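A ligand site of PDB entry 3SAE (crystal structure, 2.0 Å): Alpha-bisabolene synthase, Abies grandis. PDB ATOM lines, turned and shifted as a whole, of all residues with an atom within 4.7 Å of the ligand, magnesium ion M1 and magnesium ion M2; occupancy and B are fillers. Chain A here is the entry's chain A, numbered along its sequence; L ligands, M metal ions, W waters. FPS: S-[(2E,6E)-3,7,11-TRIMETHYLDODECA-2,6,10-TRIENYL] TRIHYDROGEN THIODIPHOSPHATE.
Water W7 binds magnesium ion M2 (2.1 Å). Magnesium ion M2 is bound by OD1 of Asp 566 (2.1 Å). Magnesium ion M2 is bound by water W6 (2.1 Å). Magnesium ion M2 is bound by OD2 of Asp 570 (2.1 Å). Water W3 binds magnesium ion M2, 2.1 Å away. O1A of the ligand is bound to magnesium ion M2 (2.1 Å). Magnesium ion M2 has six donor atoms within binding distance.
Within 4 Å of magnesium ion M2: Asp 566 and Asp 570. The nearest printed residue that does not touch magnesium ion M2 is Glu 644 (4.2 Å).
O2A of the ligand lies within salt-bridge range of NH1 of Arg 710 (2.7 Å).
The side-chain amide oxygen of Gln 669 lies close to the side-chain carboxylate of Glu 782, 2.6 Å away. The side-chain amide nitrogen of Gln 562 sits at hydrogen-bond distance from the backbone carbonyl oxygen of Gly 668, at 2.8 Å. NH2 of Arg 710 lies close to OD1 of Asp 713 (2.7 Å). The side-chain amide nitrogen (NE2) of Gln 669 sits at hydrogen-bond distance from the side-chain hydroxyl (OG) of Ser 709 (2.9 Å). NE2 of Gln 669 lies within hydrogen-bond range of OG1 of Thr 786. The side-chain hydroxyl (OH) of Tyr 641 sits close to the side-chain carboxylate (OD1) of Asp 566.
Water W2 bridges the side-chain carboxylate of Asp 567 (2.8 Å) and the side-chain carboxylate of Asp 570 (3.1 Å). Water W6 bridges the side-chain carboxylate of Glu 644 (2.6 Å) and an oxygen (O2A) of the ligand (3.3 Å). Water W8 bridges O3A of the ligand (2.6 Å) and NH2 of Arg 710 (2.9 Å).
Magnesium ion M1 is bound by O1A of the ligand, 2.0 Å away. Water W2 is bound to magnesium ion M1 (2.1 Å). Magnesium ion M1 is bound by OD2 of Asp 570 (2.1 Å). Water W1 is bound to magnesium ion M1. Water W5 binds magnesium ion M1, 2.1 Å away. OD2 of Asp 566 is bound to magnesium ion M1, at 2.1 Å. Magnesium ion M1 has six donor atoms within binding distance.
Within 4 Å of magnesium ion M1: Asp 566 and Asp 570. The nearest printed residue that does not touch magnesium ion M1 is Asp 567 (4.2 Å).
Phe 535 touches the ligand (CE1 to C15, 3.6 Å). Ala 559 touches the ligand. Gln 562 touches the ligand. Ile 667 touches the ligand. Gly 668 touches the ligand. OE1 of Gln 669 touches C9 of the ligand (3.4 Å). Leu 672 touches the ligand. Asp 713 touches the ligand (OD2 to C4, 3.6 Å). Hydrophobic or aromatic side chains within 4 Å of the ligand: Phe 535, Ile 667 and Leu 672. 11 residues have an atom within 4 Å of the ligand: Phe 535, Ala 559, Gln 562, Asp 566, Asp 570, Ile 667, Gly 668, Gln 669, Leu 672, Arg 710 and Asp 713. The nearest printed residue that does not touch the ligand is Leu 538 (4.03 Å).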
ATOM      1  N   PHE A 535       4.572   6.275 -23.562  1.00  0.00           N
ATOM      2  CA  PHE A 535       3.949   4.962 -23.678  1.00  0.00           C
ATOM      3  C   PHE A 535       4.903   3.843 -23.304  1.00  0.00           C
ATOM      4  O   PHE A 535       4.501   2.828 -22.749  1.00  0.00           O
ATOM      5  CB  PHE A 535       3.391   4.760 -25.093  1.00  0.00           C
ATOM      6  CG  PHE A 535       2.272   5.696 -25.429  1.00  0.00           C
ATOM      7  CD1 PHE A 535       1.233   5.867 -24.540  1.00  0.00           C
ATOM      8  CD2 PHE A 535       2.288   6.440 -26.586  1.00  0.00           C
ATOM      9  CE1 PHE A 535       0.199   6.742 -24.816  1.00  0.00           C
ATOM     10  CE2 PHE A 535       1.268   7.315 -26.879  1.00  0.00           C
ATOM     11  CZ  PHE A 535       0.220   7.472 -25.976  1.00  0.00           C
ATOM     12  N   LEU A 538       4.788   3.737 -19.653  1.00  0.00           N
ATOM     13  CA  LEU A 538       3.552   3.142 -19.119  1.00  0.00           C
ATOM     14  C   LEU A 538       3.726   1.639 -18.857  1.00  0.00           C
ATOM     15  O   LEU A 538       3.232   1.120 -17.857  1.00  0.00           O
ATOM     16  CB  LEU A 538       2.370   3.375 -20.066  1.00  0.00           C
ATOM     17  CG  LEU A 538       1.048   2.666 -19.753  1.00  0.00           C
ATOM     18  CD1 LEU A 538       0.391   3.131 -18.421  1.00  0.00           C
ATOM     19  CD2 LEU A 538       0.084   2.832 -20.932  1.00  0.00           C
ATOM     20  N   ALA A 559       0.505   1.514 -28.682  1.00  0.00           N
ATOM     21  CA  ALA A 559       0.061   2.739 -28.010  1.00  0.00           C
ATOM     22  C   ALA A 559       0.320   3.994 -28.867  1.00  0.00           C
ATOM     23  O   ALA A 559      -0.482   4.923 -28.875  1.00  0.00           O
ATOM     24  CB  ALA A 559       0.697   2.870 -26.629  1.00  0.00           C
ATOM     25  N   GLN A 562      -2.324   3.988 -31.489  1.00  0.00           N
ATOM     26  CA  GLN A 562      -3.607   4.308 -30.866  1.00  0.00           C
ATOM     27  C   GLN A 562      -3.824   5.794 -30.617  1.00  0.00           C
ATOM     28  O   GLN A 562      -4.922   6.307 -30.797  1.00  0.00           O
ATOM     29  CB  GLN A 562      -3.792   3.538 -29.561  1.00  0.00           C
ATOM     30  CG  GLN A 562      -4.179   2.093 -29.772  1.00  0.00           C
ATOM     31  CD  GLN A 562      -4.276   1.334 -28.480  1.00  0.00           C
ATOM     32  OE1 GLN A 562      -3.311   1.274 -27.705  1.00  0.00           O
ATOM     33  NE2 GLN A 562      -5.428   0.726 -28.245  1.00  0.00           N
ATOM     34  N   THR A 563      -2.779   6.504 -30.197  1.00  0.00           N
ATOM     35  CA  THR A 563      -2.953   7.924 -29.936  1.00  0.00           C
ATOM     36  C   THR A 563      -3.291   8.668 -31.225  1.00  0.00           C
ATOM     37  O   THR A 563      -4.040   9.634 -31.214  1.00  0.00           O
ATOM     38  CB  THR A 563      -1.729   8.574 -29.239  1.00  0.00           C
ATOM     39  OG1 THR A 563      -2.112   9.841 -28.710  1.00  0.00           O
ATOM     40  CG2 THR A 563      -0.569   8.748 -30.200  1.00  0.00           C
ATOM     41  N   ASP A 566      -6.931   7.622 -32.003  1.00  0.00           N
ATOM     42  CA  ASP A 566      -7.776   8.368 -31.083  1.00  0.00           C
ATOM     43  C   ASP A 566      -8.021   9.806 -31.556  1.00  0.00           C
ATOM     44  O   ASP A 566      -9.162  10.260 -31.649  1.00  0.00           O
ATOM     45  CB  ASP A 566      -7.161   8.362 -29.679  1.00  0.00           C
ATOM     46  CG  ASP A 566      -8.015   9.092 -28.669  1.00  0.00           C
ATOM     47  OD1 ASP A 566      -9.196   8.724 -28.512  1.00  0.00           O
ATOM     48  OD2 ASP A 566      -7.518  10.053 -28.053  1.00  0.00           O
ATOM     49  N   ASP A 567      -6.946  10.532 -31.850  1.00  0.00           N
ATOM     50  CA  ASP A 567      -7.065  11.910 -32.306  1.00  0.00           C
ATOM     51  C   ASP A 567      -7.848  11.964 -33.612  1.00  0.00           C
ATOM     52  O   ASP A 567      -8.667  12.862 -33.834  1.00  0.00           O
ATOM     53  CB  ASP A 567      -5.686  12.566 -32.475  1.00  0.00           C
ATOM     54  CG  ASP A 567      -5.003  12.853 -31.135  1.00  0.00           C
ATOM     55  OD1 ASP A 567      -5.651  12.727 -30.076  1.00  0.00           O
ATOM     56  OD2 ASP A 567      -3.807  13.214 -31.145  1.00  0.00           O
ATOM     57  N   ASP A 570     -11.759  11.150 -32.623  1.00  0.00           N
ATOM     58  CA  ASP A 570     -12.494  12.044 -31.739  1.00  0.00           C
ATOM     59  C   ASP A 570     -12.269  13.536 -32.014  1.00  0.00           C
ATOM     60  O   ASP A 570     -12.880  14.376 -31.386  1.00  0.00           O
ATOM     61  CB  ASP A 570     -12.273  11.703 -30.255  1.00  0.00           C
ATOM     62  CG  ASP A 570     -10.860  11.969 -29.790  1.00  0.00           C
ATOM     63  OD1 ASP A 570     -10.186  12.819 -30.408  1.00  0.00           O
ATOM     64  OD2 ASP A 570     -10.424  11.318 -28.803  1.00  0.00           O
ATOM     65  N   TYR A 641     -14.872   3.479 -31.329  1.00  0.00           N
ATOM     66  CA  TYR A 641     -14.541   4.851 -31.714  1.00  0.00           C
ATOM     67  C   TYR A 641     -15.564   5.446 -32.682  1.00  0.00           C
ATOM     68  O   TYR A 641     -15.950   6.605 -32.567  1.00  0.00           O
ATOM     69  CB  TYR A 641     -13.170   4.900 -32.399  1.00  0.00           C
ATOM     70  CG  TYR A 641     -11.975   5.029 -31.498  1.00  0.00           C
ATOM     71  CD1 TYR A 641     -12.107   5.383 -30.154  1.00  0.00           C
ATOM     72  CD2 TYR A 641     -10.698   4.805 -31.989  1.00  0.00           C
ATOM     73  CE1 TYR A 641     -10.986   5.489 -29.327  1.00  0.00           C
ATOM     74  CE2 TYR A 641      -9.578   4.906 -31.175  1.00  0.00           C
ATOM     75  CZ  TYR A 641      -9.724   5.252 -29.850  1.00  0.00           C
ATOM     76  OH  TYR A 641      -8.593   5.365 -29.073  1.00  0.00           O
ATOM     77  N   GLU A 644     -18.784   6.415 -31.047  1.00  0.00           N
ATOM     78  CA  GLU A 644     -18.535   7.669 -30.349  1.00  0.00           C
ATOM     79  C   GLU A 644     -18.474   8.837 -31.320  1.00  0.00           C
ATOM     80  O   GLU A 644     -18.910   9.945 -31.008  1.00  0.00           O
ATOM     81  CB  GLU A 644     -17.215   7.583 -29.585  1.00  0.00           C
ATOM     82  CG  GLU A 644     -16.818   8.892 -28.899  1.00  0.00           C
ATOM     83  CD  GLU A 644     -15.437   8.842 -28.291  1.00  0.00           C
ATOM     84  OE1 GLU A 644     -15.130   9.700 -27.428  1.00  0.00           O
ATOM     85  OE2 GLU A 644     -14.636   7.961 -28.664  1.00  0.00           O
ATOM     86  N   ILE A 667     -11.980   2.820 -25.143  1.00  0.00           N
ATOM     87  CA  ILE A 667     -10.884   3.589 -24.576  1.00  0.00           C
ATOM     88  C   ILE A 667      -9.524   3.040 -25.068  1.00  0.00           C
ATOM     89  O   ILE A 667      -8.552   3.787 -25.155  1.00  0.00           O
ATOM     90  CB  ILE A 667     -10.930   3.686 -23.031  1.00  0.00           C
ATOM     91  CG1 ILE A 667     -10.001   4.812 -22.566  1.00  0.00           C
ATOM     92  CG2 ILE A 667     -10.547   2.362 -22.387  1.00  0.00           C
ATOM     93  CD1 ILE A 667      -9.951   4.987 -21.074  1.00  0.00           C
ATOM     94  N   GLY A 668      -9.472   1.757 -25.406  1.00  0.00           N
ATOM     95  CA  GLY A 668      -8.308   1.194 -26.086  1.00  0.00           C
ATOM     96  C   GLY A 668      -7.352   0.349 -25.260  1.00  0.00           C
ATOM     97  O   GLY A 668      -6.429  -0.268 -25.812  1.00  0.00           O
ATOM     98  N   GLN A 669      -7.543   0.329 -23.945  1.00  0.00           N
ATOM     99  CA  GLN A 669      -6.678  -0.415 -23.035  1.00  0.00           C
ATOM    100  C   GLN A 669      -6.740  -1.908 -23.306  1.00  0.00           C
ATOM    101  O   GLN A 669      -5.736  -2.603 -23.208  1.00  0.00           O
ATOM    102  CB  GLN A 669      -7.034  -0.146 -21.569  1.00  0.00           C
ATOM    103  CG  GLN A 669      -6.616   1.233 -21.040  1.00  0.00           C
ATOM    104  CD  GLN A 669      -5.180   1.241 -20.527  1.00  0.00           C
ATOM    105  OE1 GLN A 669      -4.271   0.816 -21.225  1.00  0.00           O
ATOM    106  NE2 GLN A 669      -4.983   1.727 -19.310  1.00  0.00           N
ATOM    107  N   LEU A 672      -4.580  -2.908 -26.362  1.00  0.00           N
ATOM    108  CA  LEU A 672      -3.195  -2.569 -26.013  1.00  0.00           C
ATOM    109  C   LEU A 672      -2.586  -3.592 -25.048  1.00  0.00           C
ATOM    110  O   LEU A 672      -1.450  -4.048 -25.234  1.00  0.00           O
ATOM    111  CB  LEU A 672      -3.140  -1.167 -25.411  1.00  0.00           C
ATOM    112  CG  LEU A 672      -1.800  -0.687 -24.860  1.00  0.00           C
ATOM    113  CD1 LEU A 672      -0.780  -0.568 -25.983  1.00  0.00           C
ATOM    114  CD2 LEU A 672      -1.986   0.655 -24.166  1.00  0.00           C
ATOM    115  N   SER A 709      -9.686   2.918 -16.155  1.00  0.00           N
ATOM    116  CA  SER A 709      -9.013   3.914 -16.965  1.00  0.00           C
ATOM    117  C   SER A 709      -9.981   5.012 -17.428  1.00  0.00           C
ATOM    118  O   SER A 709      -9.700   6.196 -17.276  1.00  0.00           O
ATOM    119  CB  SER A 709      -8.341   3.254 -18.173  1.00  0.00           C
ATOM    120  OG  SER A 709      -7.313   2.353 -17.765  1.00  0.00           O
ATOM    121  N   ARG A 710     -11.102   4.607 -18.007  1.00  0.00           N
ATOM    122  CA  ARG A 710     -12.107   5.555 -18.479  1.00  0.00           C
ATOM    123  C   ARG A 710     -12.587   6.498 -17.366  1.00  0.00           C
ATOM    124  O   ARG A 710     -12.612   7.730 -17.534  1.00  0.00           O
ATOM    125  CB  ARG A 710     -13.304   4.806 -19.082  1.00  0.00           C
ATOM    126  CG  ARG A 710     -14.488   5.693 -19.498  1.00  0.00           C
ATOM    127  CD  ARG A 710     -14.153   6.541 -20.719  1.00  0.00           C
ATOM    128  NE  ARG A 710     -13.243   7.627 -20.396  1.00  0.00           N
ATOM    129  CZ  ARG A 710     -12.552   8.332 -21.280  1.00  0.00           C
ATOM    130  NH1 ARG A 710     -12.672   8.072 -22.581  1.00  0.00           N
ATOM    131  NH2 ARG A 710     -11.748   9.307 -20.874  1.00  0.00           N
ATOM    132  N   ASP A 713      -9.749   8.632 -15.677  1.00  0.00           N
ATOM    133  CA  ASP A 713      -9.499   9.736 -16.590  1.00  0.00           C
ATOM    134  C   ASP A 713     -10.587  10.802 -16.439  1.00  0.00           C
ATOM    135  O   ASP A 713     -10.282  11.987 -16.289  1.00  0.00           O
ATOM    136  CB  ASP A 713      -9.425   9.257 -18.041  1.00  0.00           C
ATOM    137  CG  ASP A 713      -9.360  10.411 -19.015  1.00  0.00           C
ATOM    138  OD1 ASP A 713     -10.426  11.000 -19.302  1.00  0.00           O
ATOM    139  OD2 ASP A 713      -8.258  10.734 -19.510  1.00  0.00           O
ATOM    140  N   GLU A 721     -12.281  19.590 -20.095  1.00  0.00           N
ATOM    141  CA  GLU A 721     -13.009  19.189 -21.290  1.00  0.00           C
ATOM    142  C   GLU A 721     -14.357  19.869 -21.379  1.00  0.00           C
ATOM    143  O   GLU A 721     -14.800  20.242 -22.466  1.00  0.00           O
ATOM    144  CB  GLU A 721     -13.193  17.673 -21.299  1.00  0.00           C
ATOM    145  CG  GLU A 721     -11.887  16.901 -21.301  1.00  0.00           C
ATOM    146  CD  GLU A 721     -12.064  15.459 -20.883  1.00  0.00           C
ATOM    147  OE1 GLU A 721     -11.062  14.720 -20.889  1.00  0.00           O
ATOM    148  OE2 GLU A 721     -13.206  15.076 -20.543  1.00  0.00           O
ATOM    149  N   GLU A 726     -15.974  20.203 -24.987  1.00  0.00           N
ATOM    150  CA  GLU A 726     -15.896  18.819 -25.442  1.00  0.00           C
ATOM    151  C   GLU A 726     -17.172  18.035 -25.197  1.00  0.00           C
ATOM    152  O   GLU A 726     -18.014  18.421 -24.371  1.00  0.00           O
ATOM    153  CB  GLU A 726     -14.717  18.094 -24.782  1.00  0.00           C
ATOM    154  CG  GLU A 726     -13.538  17.836 -25.713  1.00  0.00           C
ATOM    155  CD  GLU A 726     -12.411  17.064 -25.030  1.00  0.00           C
ATOM    156  OE1 GLU A 726     -12.669  15.976 -24.478  1.00  0.00           O
ATOM    157  OE2 GLU A 726     -11.263  17.563 -25.050  1.00  0.00           O
ATOM    158  N   GLU A 782       0.288  -2.350 -15.355  1.00  0.00           N
ATOM    159  CA  GLU A 782      -0.051  -1.321 -16.333  1.00  0.00           C
ATOM    160  C   GLU A 782      -1.228  -0.498 -15.787  1.00  0.00           C
ATOM    161  O   GLU A 782      -1.253   0.726 -15.892  1.00  0.00           O
ATOM    162  CB  GLU A 782      -0.370  -1.909 -17.712  1.00  0.00           C
ATOM    163  CG  GLU A 782      -0.381  -0.867 -18.871  1.00  0.00           C
ATOM    164  CD  GLU A 782      -1.779  -0.372 -19.250  1.00  0.00           C
ATOM    165  OE1 GLU A 782      -2.689  -0.388 -18.388  1.00  0.00           O
ATOM    166  OE2 GLU A 782      -1.965   0.033 -20.413  1.00  0.00           O
ATOM    167  N   THR A 786      -1.258   3.497 -14.968  1.00  0.00           N
ATOM    168  CA  THR A 786      -2.354   4.320 -15.468  1.00  0.00           C
ATOM    169  C   THR A 786      -2.986   5.119 -14.331  1.00  0.00           C
ATOM    170  O   THR A 786      -3.288   6.313 -14.488  1.00  0.00           O
ATOM    171  CB  THR A 786      -3.451   3.466 -16.154  1.00  0.00           C
ATOM    172  OG1 THR A 786      -2.863   2.704 -17.225  1.00  0.00           O
ATOM    173  CG2 THR A 786      -4.576   4.370 -16.712  1.00  0.00           C
ATOM    174  N   PHE A 790      -3.721   9.462 -13.397  1.00  0.00           N
ATOM    175  CA  PHE A 790      -5.038  10.039 -13.147  1.00  0.00           C
ATOM    176  C   PHE A 790      -5.388  10.198 -11.663  1.00  0.00           C
ATOM    177  O   PHE A 790      -6.551  10.434 -11.309  1.00  0.00           O
ATOM    178  CB  PHE A 790      -6.099   9.204 -13.859  1.00  0.00           C
ATOM    179  CG  PHE A 790      -5.897   9.130 -15.337  1.00  0.00           C
ATOM    180  CD1 PHE A 790      -5.717  10.285 -16.088  1.00  0.00           C
ATOM    181  CD2 PHE A 790      -5.878   7.911 -15.984  1.00  0.00           C
ATOM    182  CE1 PHE A 790      -5.523  10.219 -17.454  1.00  0.00           C
ATOM    183  CE2 PHE A 790      -5.682   7.848 -17.359  1.00  0.00           C
ATOM    184  CZ  PHE A 790      -5.503   9.005 -18.088  1.00  0.00           C
HETATM  185  C1  FPS L   1      -8.079   8.216 -23.971  1.00  0.00           C
HETATM  186  S1  FPS L   1      -8.077  10.009 -23.722  1.00  0.00           S
HETATM  187  C2  FPS L   1      -6.787   7.653 -23.406  1.00  0.00           C
HETATM  188  C3  FPS L   1      -6.671   7.349 -22.129  1.00  0.00           C
HETATM  189  C4  FPS L   1      -7.830   7.565 -21.185  1.00  0.00           C
HETATM  190  C5  FPS L   1      -5.340   6.873 -21.577  1.00  0.00           C
HETATM  191  C6  FPS L   1      -5.472   5.417 -21.128  1.00  0.00           C
HETATM  192  C7  FPS L   1      -5.845   4.563 -22.319  1.00  0.00           C
HETATM  193  C8  FPS L   1      -4.916   3.913 -22.980  1.00  0.00           C
HETATM  194  C10 FPS L   1      -5.303   3.036 -24.161  1.00  0.00           C
HETATM  195  C9  FPS L   1      -3.514   3.869 -22.429  1.00  0.00           C
HETATM  196  C11 FPS L   1      -4.600   3.504 -25.436  1.00  0.00           C
HETATM  197  C12 FPS L   1      -5.237   4.765 -25.971  1.00  0.00           C
HETATM  198  C13 FPS L   1      -4.484   5.797 -26.278  1.00  0.00           C
HETATM  199  C14 FPS L   1      -5.118   7.128 -26.589  1.00  0.00           C
HETATM  200  C15 FPS L   1      -2.992   5.666 -26.151  1.00  0.00           C
HETATM  201  PA  FPS L   1      -9.922  10.507 -24.625  1.00  0.00           P
HETATM  202  O1A FPS L   1      -9.794  10.504 -26.122  1.00  0.00           O
HETATM  203  O2A FPS L   1     -11.043   9.408 -24.256  1.00  0.00           O
HETATM  204  O3A FPS L   1     -10.319  11.971 -24.108  1.00  0.00           O
HETATM  205 MG    MG M   1      -8.826  11.666 -27.500  1.00  0.00          MG
HETATM  206 MG    MG M   2     -10.895   9.591 -27.703  1.00  0.00          MG
HETATM  207 MG    MG M   3     -10.712  12.896 -20.101  1.00  0.00          MG
HETATM  208  O   HOH W   1      -7.262  12.121 -26.181  1.00  0.00           O
HETATM  209  O   HOH W   2      -7.880  13.222 -28.447  1.00  0.00           O
HETATM  210  O   HOH W   3     -11.133   7.999 -26.352  1.00  0.00           O
HETATM  211  O   HOH W   4      -8.872  14.083 -23.310  1.00  0.00           O
HETATM  212  O   HOH W   5      -9.722  13.341 -26.610  1.00  0.00           O
HETATM  213  O   HOH W   6     -12.644  10.443 -26.937  1.00  0.00           O
HETATM  214  O   HOH W   7     -11.783   8.428 -29.152  1.00  0.00           O
HETATM  215  O   HOH W   8     -11.497  11.983 -21.827  1.00  0.00           O
